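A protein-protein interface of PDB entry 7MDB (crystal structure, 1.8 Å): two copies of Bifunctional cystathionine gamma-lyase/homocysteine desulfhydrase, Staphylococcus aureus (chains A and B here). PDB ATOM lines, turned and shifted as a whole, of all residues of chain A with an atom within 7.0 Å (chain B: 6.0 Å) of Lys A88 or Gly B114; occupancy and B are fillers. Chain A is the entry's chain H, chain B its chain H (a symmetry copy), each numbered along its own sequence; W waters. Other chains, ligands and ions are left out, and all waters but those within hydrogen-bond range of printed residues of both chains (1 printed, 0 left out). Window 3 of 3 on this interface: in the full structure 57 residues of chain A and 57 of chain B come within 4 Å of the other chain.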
ATOM      1  N   LEU A  86     -22.126   9.038  -2.267  1.00  0.00           N
ATOM      2  CA  LEU A  86     -21.763   8.436  -0.989  1.00  0.00           C
ATOM      3  C   LEU A  86     -22.654   8.959   0.140  1.00  0.00           C
ATOM      4  O   LEU A  86     -23.355   9.961  -0.006  1.00  0.00           O
ATOM      5  CB  LEU A  86     -20.292   8.723  -0.683  1.00  0.00           C
ATOM      6  CG  LEU A  86     -19.261   8.223  -1.698  1.00  0.00           C
ATOM      7  CD1 LEU A  86     -17.834   8.455  -1.198  1.00  0.00           C
ATOM      8  CD2 LEU A  86     -19.482   6.760  -2.042  1.00  0.00           C
ATOM      9  N   ASP A  87     -22.610   8.265   1.288  1.00  0.00           N
ATOM     10  CA  ASP A  87     -23.349   8.628   2.493  1.00  0.00           C
ATOM     11  C   ASP A  87     -22.385   8.978   3.620  1.00  0.00           C
ATOM     12  O   ASP A  87     -21.216   8.591   3.602  1.00  0.00           O
ATOM     13  CB  ASP A  87     -24.244   7.479   3.008  1.00  0.00           C
ATOM     14  CG  ASP A  87     -25.247   6.998   1.989  1.00  0.00           C
ATOM     15  OD1 ASP A  87     -25.685   7.787   1.123  1.00  0.00           O
ATOM     16  OD2 ASP A  87     -25.609   5.809   2.063  1.00  0.00           O
ATOM     17  N   LYS A  88     -22.892   9.688   4.627  1.00  0.00           N
ATOM     18  CA  LYS A  88     -22.109   9.892   5.841  1.00  0.00           C
ATOM     19  C   LYS A  88     -21.593   8.555   6.365  1.00  0.00           C
ATOM     20  O   LYS A  88     -22.284   7.536   6.297  1.00  0.00           O
ATOM     21  CB  LYS A  88     -22.942  10.596   6.912  1.00  0.00           C
ATOM     22  CG  LYS A  88     -23.984   9.726   7.584  1.00  0.00           C
ATOM     23  CD  LYS A  88     -24.448  10.351   8.892  1.00  0.00           C
ATOM     24  CE  LYS A  88     -25.257   9.358   9.722  1.00  0.00           C
ATOM     25  NZ  LYS A  88     -26.651   9.225   9.202  1.00  0.00           N
ATOM     26  N   GLY A  89     -20.347   8.552   6.838  1.00  0.00           N
ATOM     27  CA  GLY A  89     -19.680   7.334   7.255  1.00  0.00           C
ATOM     28  C   GLY A  89     -18.884   6.634   6.170  1.00  0.00           C
ATOM     29  O   GLY A  89     -18.032   5.795   6.488  1.00  0.00           O
ATOM     30  N   ASP A  90     -19.131   6.949   4.900  1.00  0.00           N
ATOM     31  CA  ASP A  90     -18.379   6.347   3.809  1.00  0.00           C
ATOM     32  C   ASP A  90     -16.994   6.981   3.688  1.00  0.00           C
ATOM     33  O   ASP A  90     -16.780   8.147   4.041  1.00  0.00           O
ATOM     34  CB  ASP A  90     -19.126   6.507   2.477  1.00  0.00           C
ATOM     35  CG  ASP A  90     -20.344   5.621   2.380  1.00  0.00           C
ATOM     36  OD1 ASP A  90     -20.549   4.771   3.284  1.00  0.00           O
ATOM     37  OD2 ASP A  90     -21.096   5.771   1.396  1.00  0.00           O
ATOM     38  N   HIS A  91     -16.069   6.214   3.117  1.00  0.00           N
ATOM     39  CA  HIS A  91     -14.668   6.588   2.979  1.00  0.00           C
ATOM     40  C   HIS A  91     -14.308   6.631   1.498  1.00  0.00           C
ATOM     41  O   HIS A  91     -14.738   5.770   0.720  1.00  0.00           O
ATOM     42  CB  HIS A  91     -13.798   5.575   3.754  1.00  0.00           C
ATOM     43  CG  HIS A  91     -12.317   5.754   3.609  1.00  0.00           C
ATOM     44  ND1 HIS A  91     -11.525   4.841   2.944  1.00  0.00           N
ATOM     45  CD2 HIS A  91     -11.469   6.678   4.125  1.00  0.00           C
ATOM     46  CE1 HIS A  91     -10.262   5.220   3.016  1.00  0.00           C
ATOM     47  NE2 HIS A  91     -10.201   6.332   3.728  1.00  0.00           N
ATOM     48  N   PHE A 110     -17.258  18.226   2.348  1.00  0.00           N
ATOM     49  CA  PHE A 110     -17.884  16.921   2.506  1.00  0.00           C
ATOM     50  C   PHE A 110     -17.501  16.242   3.808  1.00  0.00           C
ATOM     51  O   PHE A 110     -18.278  15.426   4.317  1.00  0.00           O
ATOM     52  CB  PHE A 110     -17.551  16.056   1.302  1.00  0.00           C
ATOM     53  CG  PHE A 110     -18.284  16.496   0.080  1.00  0.00           C
ATOM     54  CD1 PHE A 110     -19.644  16.257  -0.032  1.00  0.00           C
ATOM     55  CD2 PHE A 110     -17.645  17.225  -0.915  1.00  0.00           C
ATOM     56  CE1 PHE A 110     -20.354  16.697  -1.135  1.00  0.00           C
ATOM     57  CE2 PHE A 110     -18.348  17.672  -2.015  1.00  0.00           C
ATOM     58  CZ  PHE A 110     -19.700  17.411  -2.130  1.00  0.00           C
ATOM     59  N   PHE A 113     -20.047  16.551   6.346  1.00  0.00           N
ATOM     60  CA  PHE A 113     -21.186  15.677   6.147  1.00  0.00           C
ATOM     61  C   PHE A 113     -20.846  14.227   6.435  1.00  0.00           C
ATOM     62  O   PHE A 113     -21.606  13.334   6.055  1.00  0.00           O
ATOM     63  CB  PHE A 113     -21.710  15.840   4.721  1.00  0.00           C
ATOM     64  CG  PHE A 113     -22.110  17.249   4.410  1.00  0.00           C
ATOM     65  CD1 PHE A 113     -23.025  17.903   5.209  1.00  0.00           C
ATOM     66  CD2 PHE A 113     -21.533  17.936   3.368  1.00  0.00           C
ATOM     67  CE1 PHE A 113     -23.381  19.201   4.960  1.00  0.00           C
ATOM     68  CE2 PHE A 113     -21.890  19.245   3.116  1.00  0.00           C
ATOM     69  CZ  PHE A 113     -22.814  19.875   3.924  1.00  0.00           C
ATOM     70  N   GLY A 114     -19.716  13.972   7.087  1.00  0.00           N
ATOM     71  CA  GLY A 114     -19.380  12.630   7.497  1.00  0.00           C
ATOM     72  C   GLY A 114     -18.667  11.798   6.462  1.00  0.00           C
ATOM     73  O   GLY A 114     -18.413  10.615   6.719  1.00  0.00           O
ATOM     74  N   ILE A 115     -18.349  12.364   5.299  1.00  0.00           N
ATOM     75  CA  ILE A 115     -17.521  11.667   4.323  1.00  0.00           C
ATOM     76  C   ILE A 115     -16.082  11.717   4.801  1.00  0.00           C
ATOM     77  O   ILE A 115     -15.558  12.795   5.097  1.00  0.00           O
ATOM     78  CB  ILE A 115     -17.640  12.305   2.930  1.00  0.00           C
ATOM     79  CG1 ILE A 115     -19.096  12.353   2.476  1.00  0.00           C
ATOM     80  CG2 ILE A 115     -16.784  11.535   1.944  1.00  0.00           C
ATOM     81  CD1 ILE A 115     -19.718  11.013   2.387  1.00  0.00           C
ATOM     82  N   GLU A 116     -15.435  10.561   4.863  1.00  0.00           N
ATOM     83  CA  GLU A 116     -14.046  10.487   5.285  1.00  0.00           C
ATOM     84  C   GLU A 116     -13.126  10.312   4.085  1.00  0.00           C
ATOM     85  O   GLU A 116     -13.421   9.541   3.167  1.00  0.00           O
ATOM     86  CB  GLU A 116     -13.841   9.349   6.280  1.00  0.00           C
ATOM     87  CG  GLU A 116     -14.853   9.345   7.393  1.00  0.00           C
ATOM     88  CD  GLU A 116     -14.472  10.273   8.527  1.00  0.00           C
ATOM     89  OE1 GLU A 116     -13.889  11.350   8.256  1.00  0.00           O
ATOM     90  OE2 GLU A 116     -14.757   9.921   9.695  1.00  0.00           O
ATOM     91  N   ASP B  87     -23.927  21.103   9.234  1.00  0.00           N
ATOM     92  CA  ASP B  87     -23.096  19.912   9.381  1.00  0.00           C
ATOM     93  C   ASP B  87     -23.963  18.694   9.673  1.00  0.00           C
ATOM     94  O   ASP B  87     -25.102  18.815  10.125  1.00  0.00           O
ATOM     95  CB  ASP B  87     -22.086  20.034  10.544  1.00  0.00           C
ATOM     96  CG  ASP B  87     -21.162  21.219  10.413  1.00  0.00           C
ATOM     97  OD1 ASP B  87     -20.860  21.654   9.280  1.00  0.00           O
ATOM     98  OD2 ASP B  87     -20.723  21.719  11.465  1.00  0.00           O
ATOM     99  N   LYS B  88     -23.403  17.506   9.446  1.00  0.00           N
ATOM    100  CA  LYS B  88     -24.072  16.288   9.889  1.00  0.00           C
ATOM    101  C   LYS B  88     -24.452  16.403  11.363  1.00  0.00           C
ATOM    102  O   LYS B  88     -23.711  16.971  12.168  1.00  0.00           O
ATOM    103  CB  LYS B  88     -23.182  15.066   9.664  1.00  0.00           C
ATOM    104  CG  LYS B  88     -22.027  14.931  10.636  1.00  0.00           C
ATOM    105  CD  LYS B  88     -21.474  13.513  10.624  1.00  0.00           C
ATOM    106  CE  LYS B  88     -20.529  13.279  11.798  1.00  0.00           C
ATOM    107  NZ  LYS B  88     -19.187  13.886  11.544  1.00  0.00           N
ATOM    108  N   GLY B  89     -25.642  15.909  11.702  1.00  0.00           N
ATOM    109  CA  GLY B  89     -26.190  16.055  13.036  1.00  0.00           C
ATOM    110  C   GLY B  89     -27.046  17.290  13.249  1.00  0.00           C
ATOM    111  O   GLY B  89     -27.809  17.340  14.220  1.00  0.00           O
ATOM    112  N   ASP B  90     -26.945  18.288  12.373  1.00  0.00           N
ATOM    113  CA  ASP B  90     -27.764  19.486  12.490  1.00  0.00           C
ATOM    114  C   ASP B  90     -29.190  19.219  12.010  1.00  0.00           C
ATOM    115  O   ASP B  90     -29.438  18.360  11.156  1.00  0.00           O
ATOM    116  CB  ASP B  90     -27.163  20.639  11.674  1.00  0.00           C
ATOM    117  CG  ASP B  90     -25.909  21.205  12.296  1.00  0.00           C
ATOM    118  OD1 ASP B  90     -25.565  20.803  13.437  1.00  0.00           O
ATOM    119  OD2 ASP B  90     -25.269  22.054  11.646  1.00  0.00           O
ATOM    120  N   PHE B 110     -29.742  15.286   1.401  1.00  0.00           N
ATOM    121  CA  PHE B 110     -29.025  15.780   2.568  1.00  0.00           C
ATOM    122  C   PHE B 110     -29.236  14.912   3.796  1.00  0.00           C
ATOM    123  O   PHE B 110     -28.364  14.880   4.672  1.00  0.00           O
ATOM    124  CB  PHE B 110     -29.423  17.224   2.827  1.00  0.00           C
ATOM    125  CG  PHE B 110     -28.842  18.151   1.814  1.00  0.00           C
ATOM    126  CD1 PHE B 110     -27.488  18.442   1.841  1.00  0.00           C
ATOM    127  CD2 PHE B 110     -29.620  18.662   0.783  1.00  0.00           C
ATOM    128  CE1 PHE B 110     -26.920  19.264   0.884  1.00  0.00           C
ATOM    129  CE2 PHE B 110     -29.058  19.477  -0.179  1.00  0.00           C
ATOM    130  CZ  PHE B 110     -27.710  19.780  -0.133  1.00  0.00           C
ATOM    131  N   THR B 111     -30.343  14.174   3.856  1.00  0.00           N
ATOM    132  CA  THR B 111     -30.520  13.230   4.957  1.00  0.00           C
ATOM    133  C   THR B 111     -29.455  12.135   4.930  1.00  0.00           C
ATOM    134  O   THR B 111     -29.091  11.597   5.982  1.00  0.00           O
ATOM    135  CB  THR B 111     -31.930  12.632   4.904  1.00  0.00           C
ATOM    136  OG1 THR B 111     -32.184  11.881   6.095  1.00  0.00           O
ATOM    137  CG2 THR B 111     -32.040  11.699   3.725  1.00  0.00           C
ATOM    138  N   ARG B 112     -28.933  11.795   3.749  1.00  0.00           N
ATOM    139  CA  ARG B 112     -27.861  10.811   3.680  1.00  0.00           C
ATOM    140  C   ARG B 112     -26.561  11.359   4.242  1.00  0.00           C
ATOM    141  O   ARG B 112     -25.645  10.585   4.536  1.00  0.00           O
ATOM    142  CB  ARG B 112     -27.656  10.335   2.238  1.00  0.00           C
ATOM    143  CG  ARG B 112     -28.898   9.744   1.616  1.00  0.00           C
ATOM    144  CD  ARG B 112     -28.612   9.074   0.296  1.00  0.00           C
ATOM    145  NE  ARG B 112     -28.476  10.041  -0.803  1.00  0.00           N
ATOM    146  CZ  ARG B 112     -27.316  10.447  -1.306  1.00  0.00           C
ATOM    147  NH1 ARG B 112     -26.176   9.978  -0.809  1.00  0.00           N
ATOM    148  NH2 ARG B 112     -27.294  11.325  -2.316  1.00  0.00           N
ATOM    149  N   PHE B 113     -26.474  12.672   4.411  1.00  0.00           N
ATOM    150  CA  PHE B 113     -25.309  13.317   4.985  1.00  0.00           C
ATOM    151  C   PHE B 113     -25.531  13.703   6.435  1.00  0.00           C
ATOM    152  O   PHE B 113     -24.759  14.496   6.981  1.00  0.00           O
ATOM    153  CB  PHE B 113     -24.940  14.540   4.146  1.00  0.00           C
ATOM    154  CG  PHE B 113     -24.659  14.197   2.716  1.00  0.00           C
ATOM    155  CD1 PHE B 113     -23.711  13.244   2.406  1.00  0.00           C
ATOM    156  CD2 PHE B 113     -25.377  14.773   1.694  1.00  0.00           C
ATOM    157  CE1 PHE B 113     -23.461  12.894   1.106  1.00  0.00           C
ATOM    158  CE2 PHE B 113     -25.127  14.419   0.384  1.00  0.00           C
ATOM    159  CZ  PHE B 113     -24.167  13.471   0.098  1.00  0.00           C
ATOM    160  N   GLY B 114     -26.573  13.173   7.066  1.00  0.00           N
ATOM    161  CA  GLY B 114     -26.785  13.402   8.475  1.00  0.00           C
ATOM    162  C   GLY B 114     -27.545  14.657   8.818  1.00  0.00           C
ATOM    163  O   GLY B 114     -27.700  14.955  10.009  1.00  0.00           O
ATOM    164  N   ILE B 115     -28.010  15.412   7.824  1.00  0.00           N
ATOM    165  CA  ILE B 115     -28.888  16.546   8.085  1.00  0.00           C
ATOM    166  C   ILE B 115     -30.272  16.012   8.398  1.00  0.00           C
ATOM    167  O   ILE B 115     -30.829  15.225   7.627  1.00  0.00           O
ATOM    168  CB  ILE B 115     -28.946  17.498   6.880  1.00  0.00           C
ATOM    169  CG1 ILE B 115     -27.547  17.967   6.489  1.00  0.00           C
ATOM    170  CG2 ILE B 115     -29.848  18.673   7.204  1.00  0.00           C
ATOM    171  CD1 ILE B 115     -26.857  18.696   7.576  1.00  0.00           C
ATOM    172  N   GLU B 116     -30.839  16.446   9.516  1.00  0.00           N
ATOM    173  CA  GLU B 116     -32.172  16.020   9.910  1.00  0.00           C
ATOM    174  C   GLU B 116     -33.194  17.110   9.616  1.00  0.00           C
ATOM    175  O   GLU B 116     -32.946  18.295   9.857  1.00  0.00           O
ATOM    176  CB  GLU B 116     -32.208  15.646  11.388  1.00  0.00           C
ATOM    177  CG  GLU B 116     -31.092  14.721  11.792  1.00  0.00           C
ATOM    178  CD  GLU B 116     -31.415  13.267  11.517  1.00  0.00           C
ATOM    179  OE1 GLU B 116     -32.086  12.980  10.497  1.00  0.00           O
ATOM    180  OE2 GLU B 116     -30.995  12.409  12.327  1.00  0.00           O
HETATM  181  O   HOH W   1     -26.802   8.215   5.863  1.00  0.00           O
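O of Leu A86 lies within hydrogen-bond range of NH1 of Arg B112.
The side-chain carboxylate (OD1) of Asp A87 lies within salt-bridge range of the guanidinium group (NH1) of Arg B112, at 3.0 Å.
O of Arg B112 is in hydrogen-bond range of N of Lys A88 (2.9 Å).
The backbone carbonyl oxygen (O) of Phe A113 lies close to the backbone carbonyl oxygen (O) of Phe B113.
Printed residues of chain A that touch a printed residue of chain B: Leu A86, Asp A87, Lys A88, Phe A113 and Gly A114.
Among the printed residues, 7 pairs touch across the chains.
Among the printed residues, Asp or Glu carboxylates within 4 Å of a Lys or Arg side-chain nitrogen of the other chain: Asp A87 with Arg B112.
Water W1 lies within hydrogen-bond range of O of Arg B112 (3.0 Å) and NZ of Lys A88 (3.5 Å).
Phe B113 touches Leu A86 (CE1 to O, 3.1 Å).
Lys A88 touches Gly B114 (CD to CA, 3.9 Å).
Gly A114 touches Lys B88 (CA to CD, 3.9 Å).
OD2 of Asp A90 lies within hydrogen-bond range of N of Asp A87 (2.9 Å).
The backbone carbonyl oxygen (O) of Gly A114 lies within hydrogen-bond range of the backbone NH (N) of Gly A89 (2.8 Å).
The backbone NH (N) of Gly B89 is in hydrogen-bond range of the backbone carbonyl oxygen (O) of Gly B114 (2.8 Å).
Lys A88 touches Gly B114, and with the chains exchanged Gly A114 touches Lys B88.
Phe A113 touches its own counterpart, Phe B113.
Of the 7 pairs that touch across the chains among the printed residues, 3 have their exchanged pair printed and touching as well.
Of the printed residues of chain B, Phe A113 touches Phe B113 (3.5 Å).
Of the printed residues of chain A, Lys B88 touches Gly A114.
Of the printed residues of chain A, Phe B113 touches Leu A86 and Phe A113.
Of the printed residues of chain A, Gly B114 touches Lys A88 (3.9 Å).
The nearest residue of chain B that does not touch Lys A88 is Phe B113 (4.1 Å).
The nearest residue of chain A that does not touch Gly B114 is Phe A113 (5.1 Å).
The nearest printed residue of chain A that does not touch Lys B88 is Phe A113 (4.1 Å).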
